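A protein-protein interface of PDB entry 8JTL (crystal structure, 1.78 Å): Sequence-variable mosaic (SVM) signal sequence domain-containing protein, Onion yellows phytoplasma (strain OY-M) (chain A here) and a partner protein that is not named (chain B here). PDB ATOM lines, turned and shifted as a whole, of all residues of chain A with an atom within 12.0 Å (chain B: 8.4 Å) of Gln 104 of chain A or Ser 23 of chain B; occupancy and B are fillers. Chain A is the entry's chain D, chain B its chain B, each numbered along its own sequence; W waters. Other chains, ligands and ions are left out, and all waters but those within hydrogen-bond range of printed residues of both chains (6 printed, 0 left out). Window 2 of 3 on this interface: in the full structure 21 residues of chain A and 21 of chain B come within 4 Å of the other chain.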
ATOM      1  N   THR A  18      -3.579  -6.053  25.999  1.00  0.00           N
ATOM      2  CA  THR A  18      -4.978  -5.733  26.129  1.00  0.00           C
ATOM      3  C   THR A  18      -5.812  -6.597  25.213  1.00  0.00           C
ATOM      4  O   THR A  18      -5.459  -6.794  24.056  1.00  0.00           O
ATOM      5  CB  THR A  18      -5.202  -4.276  25.820  1.00  0.00           C
ATOM      6  OG1 THR A  18      -4.474  -3.518  26.792  1.00  0.00           O
ATOM      7  CG2 THR A  18      -6.639  -3.937  25.962  1.00  0.00           C
ATOM      8  N   PHE A  19      -6.893  -7.119  25.761  1.00  0.00           N
ATOM      9  CA  PHE A  19      -7.828  -7.941  25.015  1.00  0.00           C
ATOM     10  C   PHE A  19      -9.209  -7.352  25.183  1.00  0.00           C
ATOM     11  O   PHE A  19      -9.563  -6.885  26.271  1.00  0.00           O
ATOM     12  CB  PHE A  19      -7.805  -9.375  25.518  1.00  0.00           C
ATOM     13  CG  PHE A  19      -6.625 -10.142  25.003  1.00  0.00           C
ATOM     14  CD1 PHE A  19      -6.677 -10.741  23.773  1.00  0.00           C
ATOM     15  CD2 PHE A  19      -5.464 -10.217  25.742  1.00  0.00           C
ATOM     16  CE1 PHE A  19      -5.579 -11.451  23.259  1.00  0.00           C
ATOM     17  CE2 PHE A  19      -4.366 -10.898  25.236  1.00  0.00           C
ATOM     18  CZ  PHE A  19      -4.422 -11.529  24.005  1.00  0.00           C
ATOM     19  N   SER A  20     -10.041  -7.494  24.189  1.00  0.00           N
ATOM     20  CA  SER A  20     -11.413  -7.051  24.338  1.00  0.00           C
ATOM     21  C   SER A  20     -12.170  -8.107  25.124  1.00  0.00           C
ATOM     22  O   SER A  20     -13.139  -7.791  25.765  1.00  0.00           O
ATOM     23  CB  SER A  20     -12.019  -6.792  22.977  1.00  0.00           C
ATOM     24  OG  SER A  20     -11.423  -5.684  22.378  1.00  0.00           O
ATOM     25  N   ASP A  21     -11.703  -9.353  25.089  1.00  0.00           N
ATOM     26  CA  ASP A  21     -12.343 -10.460  25.814  1.00  0.00           C
ATOM     27  C   ASP A  21     -11.269 -11.322  26.463  1.00  0.00           C
ATOM     28  O   ASP A  21     -10.378 -11.763  25.784  1.00  0.00           O
ATOM     29  CB  ASP A  21     -13.164 -11.328  24.842  1.00  0.00           C
ATOM     30  CG  ASP A  21     -14.052 -12.327  25.521  1.00  0.00           C
ATOM     31  OD1 ASP A  21     -14.011 -12.494  26.750  1.00  0.00           O
ATOM     32  OD2 ASP A  21     -14.819 -12.967  24.796  1.00  0.00           O
ATOM     33  N   ILE A  22     -11.382 -11.550  27.767  1.00  0.00           N
ATOM     34  CA  ILE A  22     -10.411 -12.410  28.407  1.00  0.00           C
ATOM     35  C   ILE A  22     -10.403 -13.771  27.748  1.00  0.00           C
ATOM     36  O   ILE A  22      -9.382 -14.457  27.740  1.00  0.00           O
ATOM     37  CB  ILE A  22     -10.735 -12.502  29.908  1.00  0.00           C
ATOM     38  CG1 ILE A  22      -9.553 -13.092  30.662  1.00  0.00           C
ATOM     39  CG2 ILE A  22     -12.002 -13.312  30.159  1.00  0.00           C
ATOM     40  CD1 ILE A  22      -9.835 -13.193  32.145  1.00  0.00           C
ATOM     41  N   SER A  24     -10.272 -14.543  24.752  1.00  0.00           N
ATOM     42  CA  SER A  24      -9.253 -14.645  23.726  1.00  0.00           C
ATOM     43  C   SER A  24      -7.969 -15.239  24.275  1.00  0.00           C
ATOM     44  O   SER A  24      -7.209 -15.857  23.530  1.00  0.00           O
ATOM     45  CB  SER A  24      -8.971 -13.279  23.130  1.00  0.00           C
ATOM     46  OG  SER A  24     -10.154 -12.762  22.578  1.00  0.00           O
ATOM     47  N   HIS A  62     -10.709  -1.629  37.091  1.00  0.00           N
ATOM     48  CA  HIS A  62     -11.847  -2.346  36.535  1.00  0.00           C
ATOM     49  C   HIS A  62     -11.453  -3.081  35.249  1.00  0.00           C
ATOM     50  O   HIS A  62     -12.048  -4.107  34.912  1.00  0.00           O
ATOM     51  CB  HIS A  62     -12.982  -1.331  36.312  1.00  0.00           C
ATOM     52  CG  HIS A  62     -13.976  -1.725  35.273  1.00  0.00           C
ATOM     53  ND1 HIS A  62     -13.685  -1.782  33.930  1.00  0.00           N
ATOM     54  CD2 HIS A  62     -15.284  -2.070  35.391  1.00  0.00           C
ATOM     55  CE1 HIS A  62     -14.764  -2.162  33.264  1.00  0.00           C
ATOM     56  NE2 HIS A  62     -15.749  -2.336  34.125  1.00  0.00           N
ATOM     57  N   ASN A  63     -10.458  -2.580  34.522  1.00  0.00           N
ATOM     58  CA  ASN A  63     -10.054  -3.199  33.260  1.00  0.00           C
ATOM     59  C   ASN A  63      -8.893  -4.148  33.429  1.00  0.00           C
ATOM     60  O   ASN A  63      -8.397  -4.655  32.431  1.00  0.00           O
ATOM     61  CB  ASN A  63      -9.706  -2.132  32.205  1.00  0.00           C
ATOM     62  CG  ASN A  63      -8.489  -1.282  32.606  1.00  0.00           C
ATOM     63  OD1 ASN A  63      -8.224  -1.110  33.800  1.00  0.00           O
ATOM     64  ND2 ASN A  63      -7.781  -0.696  31.605  1.00  0.00           N
ATOM     65  N   LEU A  64      -8.479  -4.449  34.662  1.00  0.00           N
ATOM     66  CA  LEU A  64      -7.385  -5.399  34.849  1.00  0.00           C
ATOM     67  C   LEU A  64      -7.929  -6.817  34.721  1.00  0.00           C
ATOM     68  O   LEU A  64      -8.908  -7.174  35.367  1.00  0.00           O
ATOM     69  CB  LEU A  64      -6.730  -5.194  36.216  1.00  0.00           C
ATOM     70  CG  LEU A  64      -5.607  -6.206  36.443  1.00  0.00           C
ATOM     71  CD1 LEU A  64      -4.560  -5.973  35.451  1.00  0.00           C
ATOM     72  CD2 LEU A  64      -5.084  -6.100  37.885  1.00  0.00           C
ATOM     73  N   LEU A  65      -7.315  -7.621  33.856  1.00  0.00           N
ATOM     74  CA  LEU A  65      -7.736  -9.003  33.675  1.00  0.00           C
ATOM     75  C   LEU A  65      -6.883  -9.973  34.469  1.00  0.00           C
ATOM     76  O   LEU A  65      -7.374 -10.990  34.940  1.00  0.00           O
ATOM     77  CB  LEU A  65      -7.672  -9.385  32.191  1.00  0.00           C
ATOM     78  CG  LEU A  65      -8.724  -8.636  31.409  1.00  0.00           C
ATOM     79  CD1 LEU A  65      -8.629  -9.134  30.002  1.00  0.00           C
ATOM     80  CD2 LEU A  65     -10.132  -8.885  31.961  1.00  0.00           C
ATOM     81  N   TRP A 100      -5.092  -6.703  30.258  1.00  0.00           N
ATOM     82  CA  TRP A 100      -6.030  -5.623  30.428  1.00  0.00           C
ATOM     83  C   TRP A 100      -7.201  -5.877  29.519  1.00  0.00           C
ATOM     84  O   TRP A 100      -7.040  -6.409  28.423  1.00  0.00           O
ATOM     85  CB  TRP A 100      -5.433  -4.303  30.032  1.00  0.00           C
ATOM     86  CG  TRP A 100      -4.296  -3.887  30.826  1.00  0.00           C
ATOM     87  CD1 TRP A 100      -2.981  -4.000  30.483  1.00  0.00           C
ATOM     88  CD2 TRP A 100      -4.334  -3.263  32.112  1.00  0.00           C
ATOM     89  NE1 TRP A 100      -2.208  -3.426  31.477  1.00  0.00           N
ATOM     90  CE2 TRP A 100      -3.017  -2.968  32.472  1.00  0.00           C
ATOM     91  CE3 TRP A 100      -5.364  -2.889  32.977  1.00  0.00           C
ATOM     92  CZ2 TRP A 100      -2.693  -2.324  33.674  1.00  0.00           C
ATOM     93  CZ3 TRP A 100      -5.045  -2.262  34.170  1.00  0.00           C
ATOM     94  CH2 TRP A 100      -3.725  -1.993  34.513  1.00  0.00           C
ATOM     95  N   GLN A 101      -8.338  -5.402  29.930  1.00  0.00           N
ATOM     96  CA  GLN A 101      -9.511  -5.481  29.132  1.00  0.00           C
ATOM     97  C   GLN A 101      -9.693  -4.191  28.371  1.00  0.00           C
ATOM     98  O   GLN A 101      -9.631  -3.117  28.940  1.00  0.00           O
ATOM     99  CB  GLN A 101     -10.715  -5.653  30.014  1.00  0.00           C
ATOM    100  CG  GLN A 101     -12.038  -5.466  29.331  1.00  0.00           C
ATOM    101  CD  GLN A 101     -12.954  -6.619  29.582  1.00  0.00           C
ATOM    102  OE1 GLN A 101     -13.491  -6.771  30.670  1.00  0.00           O
ATOM    103  NE2 GLN A 101     -13.139  -7.438  28.578  1.00  0.00           N
ATOM    104  N   TYR A 102      -9.824  -4.302  27.088  1.00  0.00           N
ATOM    105  CA  TYR A 102     -10.161  -3.162  26.270  1.00  0.00           C
ATOM    106  C   TYR A 102     -11.546  -2.688  26.670  1.00  0.00           C
ATOM    107  O   TYR A 102     -12.488  -3.481  26.750  1.00  0.00           O
ATOM    108  CB  TYR A 102     -10.108  -3.539  24.791  1.00  0.00           C
ATOM    109  CG  TYR A 102     -10.000  -2.312  23.924  1.00  0.00           C
ATOM    110  CD1 TYR A 102     -11.115  -1.508  23.732  1.00  0.00           C
ATOM    111  CD2 TYR A 102      -8.788  -1.939  23.343  1.00  0.00           C
ATOM    112  CE1 TYR A 102     -11.062  -0.390  22.935  1.00  0.00           C
ATOM    113  CE2 TYR A 102      -8.712  -0.803  22.576  1.00  0.00           C
ATOM    114  CZ  TYR A 102      -9.869  -0.064  22.338  1.00  0.00           C
ATOM    115  OH  TYR A 102      -9.838   1.086  21.575  1.00  0.00           O
ATOM    116  N   GLU A 103     -11.661  -1.403  26.951  1.00  0.00           N
ATOM    117  CA  GLU A 103     -12.938  -0.795  27.318  1.00  0.00           C
ATOM    118  C   GLU A 103     -13.416   0.000  26.128  1.00  0.00           C
ATOM    119  O   GLU A 103     -12.892   1.080  25.844  1.00  0.00           O
ATOM    120  CB  GLU A 103     -12.787   0.124  28.514  1.00  0.00           C
ATOM    121  CG  GLU A 103     -11.953  -0.445  29.589  1.00  0.00           C
ATOM    122  CD  GLU A 103     -12.677  -0.381  30.876  1.00  0.00           C
ATOM    123  OE1 GLU A 103     -13.836  -0.859  30.951  1.00  0.00           O
ATOM    124  OE2 GLU A 103     -12.107   0.209  31.806  1.00  0.00           O
ATOM    125  N   GLN A 104     -14.419  -0.510  25.448  1.00  0.00           N
ATOM    126  CA  GLN A 104     -14.903   0.212  24.294  1.00  0.00           C
ATOM    127  C   GLN A 104     -16.014   1.157  24.719  1.00  0.00           C
ATOM    128  O   GLN A 104     -16.723   0.916  25.703  1.00  0.00           O
ATOM    129  CB  GLN A 104     -15.381  -0.752  23.210  1.00  0.00           C
ATOM    130  CG  GLN A 104     -15.576  -0.083  21.853  1.00  0.00           C
ATOM    131  CD  GLN A 104     -16.255  -0.988  20.859  1.00  0.00           C
ATOM    132  OE1 GLN A 104     -16.809  -2.018  21.235  1.00  0.00           O
ATOM    133  NE2 GLN A 104     -16.219  -0.611  19.574  1.00  0.00           N
ATOM    134  N   LYS A 105     -16.059   2.315  24.079  1.00  0.00           N
ATOM    135  CA  LYS A 105     -17.069   3.332  24.376  1.00  0.00           C
ATOM    136  C   LYS A 105     -16.951   3.882  25.766  1.00  0.00           C
ATOM    137  O   LYS A 105     -16.333   4.928  25.946  1.00  0.00           O
ATOM    138  CB  LYS A 105     -18.484   2.862  24.053  1.00  0.00           C
ATOM    139  CG  LYS A 105     -19.441   2.825  25.232  1.00  0.00           C
ATOM    140  CD  LYS A 105     -20.286   1.562  25.190  1.00  0.00           C
ATOM    141  CE  LYS A 105     -21.774   1.882  25.241  1.00  0.00           C
ATOM    142  NZ  LYS A 105     -22.514   0.945  26.132  1.00  0.00           N
ATOM    143  N   ASN B  19     -10.338   2.351  12.195  1.00  0.00           N
ATOM    144  CA  ASN B  19     -11.718   2.002  11.904  1.00  0.00           C
ATOM    145  C   ASN B  19     -12.280   1.011  12.928  1.00  0.00           C
ATOM    146  O   ASN B  19     -11.654  -0.004  13.257  1.00  0.00           O
ATOM    147  CB  ASN B  19     -11.793   1.412  10.504  1.00  0.00           C
ATOM    148  CG  ASN B  19     -13.166   1.532   9.925  1.00  0.00           C
ATOM    149  OD1 ASN B  19     -14.145   1.086  10.535  1.00  0.00           O
ATOM    150  ND2 ASN B  19     -13.266   2.150   8.748  1.00  0.00           N
ATOM    151  N   GLY B  20     -13.475   1.281  13.397  1.00  0.00           N
ATOM    152  CA  GLY B  20     -14.088   0.396  14.350  1.00  0.00           C
ATOM    153  C   GLY B  20     -14.882  -0.724  13.741  1.00  0.00           C
ATOM    154  O   GLY B  20     -15.591  -1.413  14.479  1.00  0.00           O
ATOM    155  N   ASP B  21     -14.794  -0.928  12.423  1.00  0.00           N
ATOM    156  CA  ASP B  21     -15.595  -1.971  11.797  1.00  0.00           C
ATOM    157  C   ASP B  21     -15.144  -3.349  12.261  1.00  0.00           C
ATOM    158  O   ASP B  21     -15.943  -4.287  12.281  1.00  0.00           O
ATOM    159  CB  ASP B  21     -15.548  -1.840  10.271  1.00  0.00           C
ATOM    160  CG  ASP B  21     -14.134  -1.904   9.700  1.00  0.00           C
ATOM    161  OD1 ASP B  21     -13.159  -1.903  10.475  1.00  0.00           O
ATOM    162  OD2 ASP B  21     -13.994  -1.941   8.453  1.00  0.00           O
ATOM    163  N   TYR B  22     -13.888  -3.471  12.658  1.00  0.00           N
ATOM    164  CA  TYR B  22     -13.405  -4.590  13.457  1.00  0.00           C
ATOM    165  C   TYR B  22     -13.374  -4.077  14.881  1.00  0.00           C
ATOM    166  O   TYR B  22     -12.621  -3.153  15.187  1.00  0.00           O
ATOM    167  CB  TYR B  22     -12.029  -5.050  13.022  1.00  0.00           C
ATOM    168  CG  TYR B  22     -12.032  -5.663  11.645  1.00  0.00           C
ATOM    169  CD1 TYR B  22     -12.308  -4.893  10.524  1.00  0.00           C
ATOM    170  CD2 TYR B  22     -11.758  -7.016  11.473  1.00  0.00           C
ATOM    171  CE1 TYR B  22     -12.310  -5.463   9.250  1.00  0.00           C
ATOM    172  CE2 TYR B  22     -11.777  -7.588  10.225  1.00  0.00           C
ATOM    173  CZ  TYR B  22     -12.049  -6.807   9.116  1.00  0.00           C
ATOM    174  OH  TYR B  22     -12.033  -7.389   7.859  1.00  0.00           O
ATOM    175  N   SER B  23     -14.185  -4.629  15.700  1.00  0.00           N
ATOM    176  CA  SER B  23     -14.394  -4.071  17.028  1.00  0.00           C
ATOM    177  C   SER B  23     -13.232  -4.417  17.944  1.00  0.00           C
ATOM    178  O   SER B  23     -12.775  -5.553  17.957  1.00  0.00           O
ATOM    179  CB  SER B  23     -15.675  -4.609  17.651  1.00  0.00           C
ATOM    180  OG  SER B  23     -15.921  -3.857  18.828  1.00  0.00           O
ATOM    181  N   PRO B  24     -12.756  -3.465  18.754  1.00  0.00           N
ATOM    182  CA  PRO B  24     -13.181  -2.062  18.837  1.00  0.00           C
ATOM    183  C   PRO B  24     -12.493  -1.186  17.799  1.00  0.00           C
ATOM    184  O   PRO B  24     -12.894  -0.064  17.499  1.00  0.00           O
ATOM    185  CB  PRO B  24     -12.731  -1.652  20.246  1.00  0.00           C
ATOM    186  CG  PRO B  24     -11.516  -2.462  20.467  1.00  0.00           C
ATOM    187  CD  PRO B  24     -11.751  -3.793  19.775  1.00  0.00           C
ATOM    188  N   SER B  25     -11.412  -1.711  17.259  1.00  0.00           N
ATOM    189  CA  SER B  25     -10.706  -1.047  16.188  1.00  0.00           C
ATOM    190  C   SER B  25      -9.940  -2.122  15.467  1.00  0.00           C
ATOM    191  O   SER B  25      -9.583  -3.142  16.062  1.00  0.00           O
ATOM    192  CB  SER B  25      -9.743   0.033  16.685  1.00  0.00           C
ATOM    193  OG  SER B  25      -8.665  -0.571  17.376  1.00  0.00           O
ATOM    194  N   ARG B  26      -9.712  -1.889  14.180  1.00  0.00           N
ATOM    195  CA  ARG B  26      -8.882  -2.809  13.436  1.00  0.00           C
ATOM    196  C   ARG B  26      -7.545  -2.944  14.107  1.00  0.00           C
ATOM    197  O   ARG B  26      -6.975  -4.024  14.128  1.00  0.00           O
ATOM    198  CB  ARG B  26      -8.682  -2.332  12.011  1.00  0.00           C
ATOM    199  CG  ARG B  26      -9.931  -2.452  11.229  1.00  0.00           C
ATOM    200  CD  ARG B  26      -9.801  -1.556  10.026  1.00  0.00           C
ATOM    201  NE  ARG B  26     -10.912  -1.776   9.116  1.00  0.00           N
ATOM    202  CZ  ARG B  26     -10.972  -1.263   7.900  1.00  0.00           C
ATOM    203  NH1 ARG B  26      -9.935  -0.635   7.369  1.00  0.00           N
ATOM    204  NH2 ARG B  26     -12.092  -1.397   7.199  1.00  0.00           N
ATOM    205  N   LEU B  27      -7.003  -1.831  14.608  1.00  0.00           N
ATOM    206  CA  LEU B  27      -5.726  -1.912  15.298  1.00  0.00           C
ATOM    207  C   LEU B  27      -5.803  -2.892  16.460  1.00  0.00           C
ATOM    208  O   LEU B  27      -4.925  -3.748  16.635  1.00  0.00           O
ATOM    209  CB  LEU B  27      -5.304  -0.539  15.806  1.00  0.00           C
ATOM    210  CG  LEU B  27      -3.841  -0.567  16.213  1.00  0.00           C
ATOM    211  CD1 LEU B  27      -3.042  -0.559  14.938  1.00  0.00           C
ATOM    212  CD2 LEU B  27      -3.533   0.657  17.056  1.00  0.00           C
ATOM    213  N   GLN B  28      -6.846  -2.781  17.266  1.00  0.00           N
ATOM    214  CA  GLN B  28      -6.927  -3.654  18.432  1.00  0.00           C
ATOM    215  C   GLN B  28      -7.166  -5.100  18.006  1.00  0.00           C
ATOM    216  O   GLN B  28      -6.563  -6.030  18.557  1.00  0.00           O
ATOM    217  CB  GLN B  28      -8.035  -3.196  19.366  1.00  0.00           C
ATOM    218  CG  GLN B  28      -8.242  -4.148  20.555  1.00  0.00           C
ATOM    219  CD  GLN B  28      -7.031  -4.258  21.446  1.00  0.00           C
ATOM    220  OE1 GLN B  28      -6.213  -3.333  21.539  1.00  0.00           O
ATOM    221  NE2 GLN B  28      -6.918  -5.374  22.132  1.00  0.00           N
ATOM    222  N   ALA B  29      -8.041  -5.300  17.016  1.00  0.00           N
ATOM    223  CA  ALA B  29      -8.274  -6.644  16.509  1.00  0.00           C
ATOM    224  C   ALA B  29      -6.972  -7.234  15.994  1.00  0.00           C
ATOM    225  O   ALA B  29      -6.619  -8.359  16.338  1.00  0.00           O
ATOM    226  CB  ALA B  29      -9.327  -6.611  15.398  1.00  0.00           C
ATOM    227  N   GLN B  30      -6.191  -6.428  15.268  1.00  0.00           N
ATOM    228  CA  GLN B  30      -4.899  -6.874  14.766  1.00  0.00           C
ATOM    229  C   GLN B  30      -3.941  -7.150  15.904  1.00  0.00           C
ATOM    230  O   GLN B  30      -3.233  -8.155  15.905  1.00  0.00           O
ATOM    231  CB  GLN B  30      -4.290  -5.807  13.877  1.00  0.00           C
ATOM    232  CG  GLN B  30      -3.043  -6.220  13.196  1.00  0.00           C
ATOM    233  CD  GLN B  30      -2.375  -5.032  12.510  1.00  0.00           C
ATOM    234  OE1 GLN B  30      -1.829  -5.163  11.452  1.00  0.00           O
ATOM    235  NE2 GLN B  30      -2.268  -3.920  13.222  1.00  0.00           N
ATOM    236  N   GLU B  32      -4.425  -8.067  18.860  1.00  0.00           N
ATOM    237  CA  GLU B  32      -4.702  -9.309  19.560  1.00  0.00           C
ATOM    238  C   GLU B  32      -4.292 -10.486  18.707  1.00  0.00           C
ATOM    239  O   GLU B  32      -3.672 -11.436  19.206  1.00  0.00           O
ATOM    240  CB  GLU B  32      -6.168  -9.410  19.911  1.00  0.00           C
ATOM    241  CG  GLU B  32      -6.589  -8.321  20.819  1.00  0.00           C
ATOM    242  CD  GLU B  32      -7.983  -8.536  21.327  1.00  0.00           C
ATOM    243  OE1 GLU B  32      -8.498  -9.669  21.219  1.00  0.00           O
ATOM    244  OE2 GLU B  32      -8.558  -7.575  21.872  1.00  0.00           O
ATOM    245  N   SER B 177     -14.792  -8.359   8.850  1.00  0.00           N
ATOM    246  CA  SER B 177     -15.290  -8.176  10.195  1.00  0.00           C
ATOM    247  C   SER B 177     -16.582  -8.960  10.362  1.00  0.00           C
ATOM    248  O   SER B 177     -17.321  -9.193   9.403  1.00  0.00           O
ATOM    249  CB  SER B 177     -15.509  -6.693  10.470  1.00  0.00           C
ATOM    250  OG  SER B 177     -16.439  -6.152   9.559  1.00  0.00           O
ATOM    251  N   GLY B 178     -16.834  -9.395  11.585  1.00  0.00           N
ATOM    252  CA  GLY B 178     -18.050 -10.115  11.861  1.00  0.00           C
ATOM    253  C   GLY B 178     -18.085 -10.587  13.288  1.00  0.00           C
ATOM    254  O   GLY B 178     -17.419 -10.028  14.161  1.00  0.00           O
ATOM    255  N   ALA B 179     -18.868 -11.644  13.502  1.00  0.00           N
ATOM    256  CA  ALA B 179     -19.078 -12.170  14.842  1.00  0.00           C
ATOM    257  C   ALA B 179     -17.782 -12.670  15.455  1.00  0.00           C
ATOM    258  O   ALA B 179     -17.632 -12.670  16.681  1.00  0.00           O
ATOM    259  CB  ALA B 179     -20.111 -13.299  14.813  1.00  0.00           C
ATOM    260  N   ASN B 180     -16.861 -13.141  14.630  1.00  0.00           N
ATOM    261  CA  ASN B 180     -15.597 -13.652  15.108  1.00  0.00           C
ATOM    262  C   ASN B 180     -14.581 -12.528  15.062  1.00  0.00           C
ATOM    263  O   ASN B 180     -14.538 -11.750  14.100  1.00  0.00           O
ATOM    264  CB  ASN B 180     -15.125 -14.810  14.243  1.00  0.00           C
ATOM    265  CG  ASN B 180     -15.880 -16.083  14.522  1.00  0.00           C
ATOM    266  OD1 ASN B 180     -16.422 -16.276  15.611  1.00  0.00           O
ATOM    267  ND2 ASN B 180     -15.957 -16.945  13.515  1.00  0.00           N
ATOM    268  N   ALA B 181     -13.786 -12.430  16.125  1.00  0.00           N
ATOM    269  CA  ALA B 181     -12.620 -11.566  16.080  1.00  0.00           C
ATOM    270  C   ALA B 181     -11.647 -12.066  15.023  1.00  0.00           C
ATOM    271  O   ALA B 181     -11.526 -13.267  14.771  1.00  0.00           O
ATOM    272  CB  ALA B 181     -11.930 -11.540  17.438  1.00  0.00           C
ATOM    273  N   LEU B 182     -10.931 -11.123  14.433  1.00  0.00           N
ATOM    274  CA  LEU B 182      -9.836 -11.446  13.534  1.00  0.00           C
ATOM    275  C   LEU B 182      -8.998 -12.608  14.048  1.00  0.00           C
ATOM    276  O   LEU B 182      -8.760 -13.582  13.332  1.00  0.00           O
ATOM    277  CB  LEU B 182      -8.989 -10.189  13.373  1.00  0.00           C
ATOM    278  CG  LEU B 182      -7.718 -10.393  12.580  1.00  0.00           C
ATOM    279  CD1 LEU B 182      -8.073 -10.934  11.191  1.00  0.00           C
ATOM    280  CD2 LEU B 182      -6.991  -9.036  12.491  1.00  0.00           C
HETATM  281  O   HOH W   1      -9.398 -11.297  19.604  1.00  0.00           O
HETATM  282  O   HOH W   2     -16.252  -0.688  17.157  1.00  0.00           O
HETATM  283  O   HOH W   3     -10.583  -6.745  19.890  1.00  0.00           O
HETATM  284  O   HOH W   4      -8.087   0.704  19.490  1.00  0.00           O
HETATM  285  O   HOH W   5     -14.048   1.813  19.411  1.00  0.00           O
HETATM  286  O   HOH W   6     -10.449 -10.248  22.729  1.00  0.00           O
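N of Ser 20 of chain A sits at hydrogen-bond distance from OE2 of Glu 32 of chain B (2.8 Å). NE2 of Gln 28 of chain B sits at hydrogen-bond distance from O of Thr 18 of chain A, at 2.8 Å. The side-chain hydroxyl of Ser 23 of chain B is in hydrogen-bond range of the side-chain amide oxygen of Gln 104 of chain A (3.2 Å).
NE2 of Gln 101 of chain A lies within hydrogen-bond range of O of Ser 20 of chain A, 2.8 Å away. O of Trp 100 of chain A is in hydrogen-bond range of N of Phe 19 of chain A, at 2.8 Å. The backbone carbonyl oxygen (O) of Asp 21 of chain A lies close to the side-chain hydroxyl (OG) of Ser 24 of chain A. The backbone NH of Gln 28 of chain B sits at hydrogen-bond distance from the side-chain hydroxyl of Ser 25 of chain B, 2.9 Å away. The side-chain amide nitrogen of Gln 28 of chain B sits at hydrogen-bond distance from the side-chain carboxylate of Glu 32 of chain B (2.8 Å). The backbone carbonyl oxygen of Phe 19 of chain A is in hydrogen-bond range of the backbone NH of Tyr 102 of chain A, 2.7 Å away.
Thr 18 of chain A touches Glu 32 of chain B (O to CG, 3.8 Å). CA of Phe 19 of chain A touches NE2 of Gln 28 of chain B (3.97 Å). Phe 19 of chain A touches Glu 32 of chain B (CA to OE2, 3.2 Å). OG of Ser 20 of chain A touches CD of Pro 24 of chain B, 3.2 Å away. Ser 20 of chain A touches Gln 28 of chain B. Glu 32 of chain B touches Ser 24 of chain A. CG of Pro 24 of chain B touches CE1 of Tyr 102 of chain A, 3.3 Å away. OE1 of Gln 28 of chain B touches CD2 of Tyr 102 of chain A (3.4 Å). NE2 of Gln 104 of chain A touches CA of Pro 24 of chain B, 3.4 Å away.
Of chain B, only Ser 23 (3.2 Å) and Pro 24 (3.4 Å) come within 4 Å of Gln 104 of chain A. Ser 23 of chain B touches one residue of chain A. No residue of chain A comes within 4 Å of Gly 20 of chain B. Asp 21 of chain B touches none of the printed residues of chain A. Pro 24 of chain B touches just these residues of chain A: Ser 20 (3.2 Å), Tyr 102 (3.3 Å) and Gln 104 (3.4 Å). No residue of chain A comes within 4 Å of Ser 25 of chain B. Gln 28 of chain B touches four residues of chain A. No residue of chain A comes within 4 Å of Ala 29 of chain B. Printed residues of chain B within 4 Å of Ser 20 of chain A: Pro 24 (3.2 Å), Gln 28 (3.98 Å) and Glu 32 (2.8 Å). Printed residues of chain B within 4 Å of Phe 19 of chain A: Gln 28 (3.97 Å) and Glu 32 (3.2 Å). Of the printed residues of chain B, Ser 24 of chain A touches Glu 32 (3.8 Å). The nearest residue of chain A that does not touch Ser 23 of chain B is Ser 20 of chain A (4.6 Å). The nearest printed residue of chain B that does not touch Ser 20 of chain A is Ser 23 of chain B (4.6 Å).
Of the 16 printed residues of chain A, 6 touch a printed residue of chain B. Hydrophobic or aromatic side chains of chain A that line the printed part of chain B: Phe 19 and Tyr 102. Of the 19 printed residues of chain B, 4 touch a printed residue of chain A. Printed residues of chain B that touch a printed residue of chain A: Ser 23, Pro 24, Gln 28 and Glu 32. Hydrophobic or aromatic side chains of chain B that line the printed part of chain A: Pro 24. Among the printed residues, 12 pairs touch across the chains.
Water W2 lies within hydrogen-bond range of NE2 of Gln 104 of chain A, O of Gly 20 of chain B and O of Pro 24 of chain B. Water W1 bridges OE1 of Glu 32 of chain B (2.5 Å) and OG of Ser 24 of chain A (3.4 Å). Water W6 lies within hydrogen-bond range of the side-chain carboxylate of Glu 32 of chain B (2.5 Å), the side-chain hydroxyl of Ser 24 of chain A (2.5 Å), the backbone NH of Asp 21 of chain A (2.8 Å) and the backbone NH of Ser 20 of chain A (3.1 Å). Water W4 bridges OG of Ser 25 of chain B (2.5 Å) and OH of Tyr 102 of chain A (2.7 Å). Water W3 lies within hydrogen-bond range of the side-chain hydroxyl of Ser 20 of chain A (2.8 Å), the side-chain carboxylate of Glu 32 of chain B (3.0 Å) and the backbone carbonyl oxygen of Ser 23 of chain B (3.2 Å). Water W5 bridges O of Pro 24 of chain B (2.9 Å) and NE2 of Gln 104 of chain A (3.3 Å).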
